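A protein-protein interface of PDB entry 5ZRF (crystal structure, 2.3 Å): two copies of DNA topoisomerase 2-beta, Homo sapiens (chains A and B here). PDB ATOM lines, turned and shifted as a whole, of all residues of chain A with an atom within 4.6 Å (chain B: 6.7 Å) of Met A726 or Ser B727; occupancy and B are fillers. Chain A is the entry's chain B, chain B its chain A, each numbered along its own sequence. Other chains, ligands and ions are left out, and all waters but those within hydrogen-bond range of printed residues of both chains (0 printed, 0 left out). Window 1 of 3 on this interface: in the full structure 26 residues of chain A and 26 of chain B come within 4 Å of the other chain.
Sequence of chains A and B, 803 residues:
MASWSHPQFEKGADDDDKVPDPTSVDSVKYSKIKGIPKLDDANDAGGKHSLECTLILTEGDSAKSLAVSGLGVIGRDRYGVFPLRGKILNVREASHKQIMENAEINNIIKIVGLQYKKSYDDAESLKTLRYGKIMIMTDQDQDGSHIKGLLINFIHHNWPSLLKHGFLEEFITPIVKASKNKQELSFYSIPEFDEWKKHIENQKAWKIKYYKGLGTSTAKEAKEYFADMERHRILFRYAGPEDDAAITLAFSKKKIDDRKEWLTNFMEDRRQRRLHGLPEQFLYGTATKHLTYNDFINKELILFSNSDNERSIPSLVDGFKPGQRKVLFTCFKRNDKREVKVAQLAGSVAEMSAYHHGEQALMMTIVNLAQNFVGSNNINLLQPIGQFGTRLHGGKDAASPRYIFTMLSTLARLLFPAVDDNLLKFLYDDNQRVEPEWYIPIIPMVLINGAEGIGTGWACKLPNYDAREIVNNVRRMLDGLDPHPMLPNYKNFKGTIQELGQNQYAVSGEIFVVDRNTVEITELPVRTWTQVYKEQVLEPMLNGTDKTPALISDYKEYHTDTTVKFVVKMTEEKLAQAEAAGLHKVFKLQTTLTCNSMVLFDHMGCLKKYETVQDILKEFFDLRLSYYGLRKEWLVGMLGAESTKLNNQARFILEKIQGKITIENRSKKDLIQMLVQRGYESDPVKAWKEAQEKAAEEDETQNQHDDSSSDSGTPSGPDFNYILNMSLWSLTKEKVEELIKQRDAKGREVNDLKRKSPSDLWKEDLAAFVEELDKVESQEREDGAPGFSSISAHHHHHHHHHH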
ATOM      1  N   GLN A 649      -5.511  25.715  11.141  1.00  0.00           N
ATOM      2  CA  GLN A 649      -6.331  24.968  10.193  1.00  0.00           C
ATOM      3  C   GLN A 649      -6.124  25.475   8.768  1.00  0.00           C
ATOM      4  O   GLN A 649      -5.954  24.679   7.835  1.00  0.00           O
ATOM      5  CB  GLN A 649      -7.806  25.056  10.588  1.00  0.00           C
ATOM      6  CG  GLN A 649      -8.177  24.259  11.831  1.00  0.00           C
ATOM      7  CD  GLN A 649      -9.611  24.498  12.270  1.00  0.00           C
ATOM      8  OE1 GLN A 649     -10.128  25.604  12.143  1.00  0.00           O
ATOM      9  NE2 GLN A 649     -10.259  23.461  12.791  1.00  0.00           N
ATOM     10  N   ILE A 653      -4.470  23.357   5.578  1.00  0.00           N
ATOM     11  CA  ILE A 653      -5.207  23.204   4.324  1.00  0.00           C
ATOM     12  C   ILE A 653      -4.385  23.738   3.149  1.00  0.00           C
ATOM     13  O   ILE A 653      -4.292  23.100   2.093  1.00  0.00           O
ATOM     14  CB  ILE A 653      -6.581  23.893   4.424  1.00  0.00           C
ATOM     15  CG1 ILE A 653      -7.485  23.145   5.405  1.00  0.00           C
ATOM     16  CG2 ILE A 653      -7.269  23.950   3.068  1.00  0.00           C
ATOM     17  CD1 ILE A 653      -7.585  21.653   5.126  1.00  0.00           C
ATOM     18  N   TYR A 722      -8.304  18.859  16.014  1.00  0.00           N
ATOM     19  CA  TYR A 722      -9.067  19.954  15.424  1.00  0.00           C
ATOM     20  C   TYR A 722      -8.675  20.202  13.974  1.00  0.00           C
ATOM     21  O   TYR A 722      -9.419  20.872  13.244  1.00  0.00           O
ATOM     22  CB  TYR A 722      -8.879  21.224  16.246  1.00  0.00           C
ATOM     23  CG  TYR A 722      -7.519  21.865  16.082  1.00  0.00           C
ATOM     24  CD1 TYR A 722      -6.391  21.331  16.698  1.00  0.00           C
ATOM     25  CD2 TYR A 722      -7.367  23.017  15.324  1.00  0.00           C
ATOM     26  CE1 TYR A 722      -5.148  21.925  16.550  1.00  0.00           C
ATOM     27  CE2 TYR A 722      -6.138  23.619  15.180  1.00  0.00           C
ATOM     28  CZ  TYR A 722      -5.031  23.071  15.794  1.00  0.00           C
ATOM     29  OH  TYR A 722      -3.810  23.681  15.647  1.00  0.00           O
ATOM     30  N   ILE A 723      -7.528  19.673  13.548  1.00  0.00           N
ATOM     31  CA  ILE A 723      -7.072  19.754  12.169  1.00  0.00           C
ATOM     32  C   ILE A 723      -7.541  18.514  11.422  1.00  0.00           C
ATOM     33  O   ILE A 723      -8.293  18.610  10.445  1.00  0.00           O
ATOM     34  CB  ILE A 723      -5.542  19.897  12.097  1.00  0.00           C
ATOM     35  CG1 ILE A 723      -5.093  21.220  12.725  1.00  0.00           C
ATOM     36  CG2 ILE A 723      -5.057  19.769  10.659  1.00  0.00           C
ATOM     37  CD1 ILE A 723      -3.597  21.393  12.736  1.00  0.00           C
ATOM     38  N   LEU A 724      -7.091  17.344  11.872  1.00  0.00           N
ATOM     39  CA  LEU A 724      -7.345  16.096  11.160  1.00  0.00           C
ATOM     40  C   LEU A 724      -8.798  15.631  11.217  1.00  0.00           C
ATOM     41  O   LEU A 724      -9.163  14.739  10.443  1.00  0.00           O
ATOM     42  CB  LEU A 724      -6.423  15.008  11.709  1.00  0.00           C
ATOM     43  CG  LEU A 724      -4.970  15.369  11.422  1.00  0.00           C
ATOM     44  CD1 LEU A 724      -4.007  14.498  12.202  1.00  0.00           C
ATOM     45  CD2 LEU A 724      -4.732  15.249   9.932  1.00  0.00           C
ATOM     46  N   ASN A 725      -9.634  16.198  12.097  1.00  0.00           N
ATOM     47  CA  ASN A 725     -11.064  15.898  12.071  1.00  0.00           C
ATOM     48  C   ASN A 725     -11.801  16.622  10.954  1.00  0.00           C
ATOM     49  O   ASN A 725     -12.964  16.292  10.692  1.00  0.00           O
ATOM     50  CB  ASN A 725     -11.743  16.263  13.397  1.00  0.00           C
ATOM     51  CG  ASN A 725     -11.455  15.266  14.504  1.00  0.00           C
ATOM     52  OD1 ASN A 725     -10.927  14.180  14.264  1.00  0.00           O
ATOM     53  ND2 ASN A 725     -11.817  15.631  15.730  1.00  0.00           N
ATOM     54  N   MET A 726     -11.176  17.601  10.307  1.00  0.00           N
ATOM     55  CA  MET A 726     -11.840  18.305   9.218  1.00  0.00           C
ATOM     56  C   MET A 726     -12.168  17.340   8.086  1.00  0.00           C
ATOM     57  O   MET A 726     -11.436  16.381   7.822  1.00  0.00           O
ATOM     58  CB  MET A 726     -10.965  19.452   8.704  1.00  0.00           C
ATOM     59  CG  MET A 726     -10.691  20.533   9.743  1.00  0.00           C
ATOM     60  SD  MET A 726      -9.451  21.747   9.205  1.00  0.00           S
ATOM     61  CE  MET A 726     -10.436  22.758   8.110  1.00  0.00           C
ATOM     62  N   SER A 727     -13.294  17.593   7.428  1.00  0.00           N
ATOM     63  CA  SER A 727     -13.751  16.717   6.360  1.00  0.00           C
ATOM     64  C   SER A 727     -12.861  16.861   5.129  1.00  0.00           C
ATOM     65  O   SER A 727     -12.179  17.871   4.930  1.00  0.00           O
ATOM     66  CB  SER A 727     -15.197  17.034   5.984  1.00  0.00           C
ATOM     67  OG  SER A 727     -15.279  18.306   5.361  1.00  0.00           O
ATOM     68  N   LEU A 728     -12.877  15.824   4.292  1.00  0.00           N
ATOM     69  CA  LEU A 728     -12.193  15.902   3.006  1.00  0.00           C
ATOM     70  C   LEU A 728     -12.693  17.072   2.168  1.00  0.00           C
ATOM     71  O   LEU A 728     -11.933  17.616   1.360  1.00  0.00           O
ATOM     72  CB  LEU A 728     -12.366  14.591   2.242  1.00  0.00           C
ATOM     73  CG  LEU A 728     -11.628  13.387   2.829  1.00  0.00           C
ATOM     74  CD1 LEU A 728     -12.209  12.101   2.260  1.00  0.00           C
ATOM     75  CD2 LEU A 728     -10.147  13.489   2.492  1.00  0.00           C
ATOM     76  N   SER A 730     -12.888  19.968   3.018  1.00  0.00           N
ATOM     77  CA  SER A 730     -12.041  21.111   3.342  1.00  0.00           C
ATOM     78  C   SER A 730     -10.951  21.356   2.313  1.00  0.00           C
ATOM     79  O   SER A 730     -10.405  22.459   2.263  1.00  0.00           O
ATOM     80  CB  SER A 730     -11.389  20.904   4.704  1.00  0.00           C
ATOM     81  OG  SER A 730     -12.355  20.566   5.672  1.00  0.00           O
ATOM     82  N   LEU A 739     -12.634  28.890   4.455  1.00  0.00           N
ATOM     83  CA  LEU A 739     -11.796  28.835   5.648  1.00  0.00           C
ATOM     84  C   LEU A 739     -10.919  30.078   5.785  1.00  0.00           C
ATOM     85  O   LEU A 739     -10.750  30.604   6.889  1.00  0.00           O
ATOM     86  CB  LEU A 739     -10.933  27.577   5.616  1.00  0.00           C
ATOM     87  CG  LEU A 739      -9.985  27.407   6.799  1.00  0.00           C
ATOM     88  CD1 LEU A 739     -10.787  27.434   8.093  1.00  0.00           C
ATOM     89  CD2 LEU A 739      -9.219  26.108   6.671  1.00  0.00           C
ATOM     90  N   ILE B 653     -10.635   6.043  -0.668  1.00  0.00           N
ATOM     91  CA  ILE B 653      -9.468   6.203   0.195  1.00  0.00           C
ATOM     92  C   ILE B 653      -8.238   5.561  -0.438  1.00  0.00           C
ATOM     93  O   ILE B 653      -7.145   6.142  -0.431  1.00  0.00           O
ATOM     94  CB  ILE B 653      -9.756   5.624   1.593  1.00  0.00           C
ATOM     95  CG1 ILE B 653     -10.801   6.476   2.318  1.00  0.00           C
ATOM     96  CG2 ILE B 653      -8.469   5.507   2.408  1.00  0.00           C
ATOM     97  CD1 ILE B 653     -10.367   7.894   2.579  1.00  0.00           C
ATOM     98  N   ILE B 723     -18.671  10.166   1.398  1.00  0.00           N
ATOM     99  CA  ILE B 723     -17.245  10.056   1.120  1.00  0.00           C
ATOM    100  C   ILE B 723     -16.552  11.306   1.637  1.00  0.00           C
ATOM    101  O   ILE B 723     -15.670  11.229   2.495  1.00  0.00           O
ATOM    102  CB  ILE B 723     -16.975   9.848  -0.381  1.00  0.00           C
ATOM    103  CG1 ILE B 723     -17.615   8.537  -0.857  1.00  0.00           C
ATOM    104  CG2 ILE B 723     -15.476   9.875  -0.659  1.00  0.00           C
ATOM    105  CD1 ILE B 723     -17.589   8.348  -2.373  1.00  0.00           C
ATOM    106  N   LEU B 724     -16.933  12.463   1.090  1.00  0.00           N
ATOM    107  CA  LEU B 724     -16.197  13.700   1.322  1.00  0.00           C
ATOM    108  C   LEU B 724     -16.361  14.270   2.726  1.00  0.00           C
ATOM    109  O   LEU B 724     -15.567  15.141   3.110  1.00  0.00           O
ATOM    110  CB  LEU B 724     -16.611  14.731   0.278  1.00  0.00           C
ATOM    111  CG  LEU B 724     -16.254  14.219  -1.123  1.00  0.00           C
ATOM    112  CD1 LEU B 724     -16.867  15.076  -2.199  1.00  0.00           C
ATOM    113  CD2 LEU B 724     -14.744  14.228  -1.265  1.00  0.00           C
ATOM    114  N   ASN B 725     -17.362  13.816   3.490  1.00  0.00           N
ATOM    115  CA  ASN B 725     -17.460  14.152   4.910  1.00  0.00           C
ATOM    116  C   ASN B 725     -16.516  13.339   5.783  1.00  0.00           C
ATOM    117  O   ASN B 725     -16.355  13.676   6.960  1.00  0.00           O
ATOM    118  CB  ASN B 725     -18.883  13.939   5.445  1.00  0.00           C
ATOM    119  CG  ASN B 725     -19.884  14.922   4.873  1.00  0.00           C
ATOM    120  OD1 ASN B 725     -19.512  15.942   4.304  1.00  0.00           O
ATOM    121  ND2 ASN B 725     -21.169  14.618   5.033  1.00  0.00           N
ATOM    122  N   MET B 726     -15.914  12.271   5.263  1.00  0.00           N
ATOM    123  CA  MET B 726     -14.913  11.546   6.035  1.00  0.00           C
ATOM    124  C   MET B 726     -13.815  12.505   6.480  1.00  0.00           C
ATOM    125  O   MET B 726     -13.431  13.418   5.745  1.00  0.00           O
ATOM    126  CB  MET B 726     -14.318  10.397   5.210  1.00  0.00           C
ATOM    127  CG  MET B 726     -15.312   9.271   4.902  1.00  0.00           C
ATOM    128  SD  MET B 726     -14.539   7.803   4.169  1.00  0.00           S
ATOM    129  CE  MET B 726     -14.077   8.414   2.553  1.00  0.00           C
ATOM    130  N   SER B 727     -13.331  12.312   7.701  1.00  0.00           N
ATOM    131  CA  SER B 727     -12.281  13.161   8.240  1.00  0.00           C
ATOM    132  C   SER B 727     -10.956  12.918   7.517  1.00  0.00           C
ATOM    133  O   SER B 727     -10.739  11.878   6.891  1.00  0.00           O
ATOM    134  CB  SER B 727     -12.102  12.901   9.733  1.00  0.00           C
ATOM    135  OG  SER B 727     -11.736  11.548   9.945  1.00  0.00           O
ATOM    136  N   LEU B 728     -10.058  13.903   7.618  1.00  0.00           N
ATOM    137  CA  LEU B 728      -8.699  13.740   7.102  1.00  0.00           C
ATOM    138  C   LEU B 728      -7.966  12.579   7.762  1.00  0.00           C
ATOM    139  O   LEU B 728      -7.039  12.027   7.160  1.00  0.00           O
ATOM    140  CB  LEU B 728      -7.896  15.032   7.291  1.00  0.00           C
ATOM    141  CG  LEU B 728      -8.427  16.284   6.589  1.00  0.00           C
ATOM    142  CD1 LEU B 728      -7.709  17.529   7.061  1.00  0.00           C
ATOM    143  CD2 LEU B 728      -8.239  16.142   5.099  1.00  0.00           C
ATOM    144  N   TRP B 729      -8.349  12.206   8.987  1.00  0.00           N
ATOM    145  CA  TRP B 729      -7.795  11.007   9.610  1.00  0.00           C
ATOM    146  C   TRP B 729      -7.962   9.780   8.724  1.00  0.00           C
ATOM    147  O   TRP B 729      -7.170   8.836   8.820  1.00  0.00           O
ATOM    148  CB  TRP B 729      -8.462  10.735  10.961  1.00  0.00           C
ATOM    149  CG  TRP B 729      -7.923  11.510  12.140  1.00  0.00           C
ATOM    150  CD1 TRP B 729      -8.598  12.423  12.900  1.00  0.00           C
ATOM    151  CD2 TRP B 729      -6.609  11.408  12.710  1.00  0.00           C
ATOM    152  NE1 TRP B 729      -7.779  12.907  13.898  1.00  0.00           N
ATOM    153  CE2 TRP B 729      -6.556  12.298  13.803  1.00  0.00           C
ATOM    154  CE3 TRP B 729      -5.475  10.652  12.401  1.00  0.00           C
ATOM    155  CZ2 TRP B 729      -5.414  12.452  14.584  1.00  0.00           C
ATOM    156  CZ3 TRP B 729      -4.338  10.812  13.178  1.00  0.00           C
ATOM    157  CH2 TRP B 729      -4.318  11.700  14.257  1.00  0.00           C
ATOM    158  N   SER B 730      -8.991   9.770   7.867  1.00  0.00           N
ATOM    159  CA  SER B 730      -9.283   8.601   7.036  1.00  0.00           C
ATOM    160  C   SER B 730      -8.119   8.228   6.132  1.00  0.00           C
ATOM    161  O   SER B 730      -8.001   7.066   5.729  1.00  0.00           O
ATOM    162  CB  SER B 730     -10.521   8.857   6.179  1.00  0.00           C
ATOM    163  OG  SER B 730     -11.589   9.333   6.974  1.00  0.00           O
ATOM    164  N   LEU B 731      -7.263   9.192   5.789  1.00  0.00           N
ATOM    165  CA  LEU B 731      -6.149   8.927   4.888  1.00  0.00           C
ATOM    166  C   LEU B 731      -4.938   8.346   5.598  1.00  0.00           C
ATOM    167  O   LEU B 731      -3.995   7.926   4.920  1.00  0.00           O
ATOM    168  CB  LEU B 731      -5.746  10.211   4.157  1.00  0.00           C
ATOM    169  CG  LEU B 731      -6.899  10.990   3.512  1.00  0.00           C
ATOM    170  CD1 LEU B 731      -6.409  12.331   2.973  1.00  0.00           C
ATOM    171  CD2 LEU B 731      -7.566  10.183   2.415  1.00  0.00           C
ATOM    172  N   LYS B 735      -6.168   4.179   9.974  1.00  0.00           N
ATOM    173  CA  LYS B 735      -7.556   4.363   9.568  1.00  0.00           C
ATOM    174  C   LYS B 735      -7.849   3.686   8.234  1.00  0.00           C
ATOM    175  O   LYS B 735      -8.960   3.185   8.030  1.00  0.00           O
ATOM    176  CB  LYS B 735      -7.890   5.854   9.497  1.00  0.00           C
ATOM    177  CG  LYS B 735      -8.034   6.527  10.859  1.00  0.00           C
ATOM    178  CD  LYS B 735      -9.240   5.979  11.591  1.00  0.00           C
ATOM    179  CE  LYS B 735      -9.454   6.651  12.927  1.00  0.00           C
ATOM    180  NZ  LYS B 735     -10.805   6.294  13.452  1.00  0.00           N
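The backbone NH (N) of Leu B728 lies within hydrogen-bond range of the backbone carbonyl oxygen (O) of Leu A724, 3.1 Å away.
N of Leu A728 sits at hydrogen-bond distance from O of Leu B724, 3.0 Å away.
The indole nitrogen (NE1) of Trp B729 sits close to the side-chain amide oxygen (OD1) of Asn A725.
N of Leu B728 sits at hydrogen-bond distance from O of Met A726 (2.8 Å).
N of Leu A728 lies within hydrogen-bond range of O of Met B726 (2.9 Å).
The backbone NH (N) of Trp B729 lies within hydrogen-bond range of the backbone carbonyl oxygen (O) of Leu A724 (3.0 Å).
The backbone carbonyl oxygen of Ser B727 is in hydrogen-bond range of the side-chain hydroxyl of Ser B730.
The backbone carbonyl oxygen (O) of Ser A727 sits at hydrogen-bond distance from the side-chain hydroxyl (OG) of Ser A730, at 2.8 Å.
Leu B728 touches Ile A723 (CD1 to O, 3.6 Å).
Leu A724 touches Ser B727.
Ser B727 touches Asn A725 (CB to O, 3.6 Å).
Met A726 touches Ser B727 (O to CA, 3.4 Å).
Ser A727 touches Leu B724.
CB of Ser A727 touches O of Asn B725 (3.7 Å).
Ser A727 touches Met B726.
Ile B723 touches Leu A728.
Leu A728 touches Leu B731.
Of chain B, only Ser B727 and Leu B728 come within 4 Å of Met A726.
Ser B727 touches just these residues of chain A: Leu A724 (3.5 Å), Asn A725 (3.6 Å) and Met A726 (3.4 Å).
Printed residues of chain A within 4 Å of Leu B731: Leu A728 (3.9 Å).
Printed residues of chain B within 4 Å of Ile A723: Leu B728 (3.6 Å).
Printed residues of chain A within 4 Å of Leu B724: Ser A727 (3.5 Å) and Leu A728 (3.0 Å).
Of the printed residues of chain A, Met B726 touches Ser A727 and Leu A728.
Ser A730 touches none of the printed residues of chain B.
The nearest printed residue of chain B that does not touch Leu A728 is Leu B728 (4.2 Å).
Along chain B the printed residues that touch a printed residue of chain A span positions 723 to 731.
Of the 11 printed residues of chain A, 6 touch a printed residue of chain B.
Among the printed residues, 15 pairs touch across the chains.
Among the printed residues, no Asp or Glu carboxylate lies within 4 Å of a Lys or Arg side-chain nitrogen of the other chain.
Ile A723 touches Leu B728, and with the chains exchanged Leu A728 touches Ile B723.
Asn A725 touches Ser B727, and with the chains exchanged Ser A727 touches Asn B725.
Met A726 touches Ser B727, and with the chains exchanged Ser A727 touches Met B726.
Met A726 touches Leu B728, and with the chains exchanged Leu A728 touches Met B726.
8 positions are printed for both chains.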
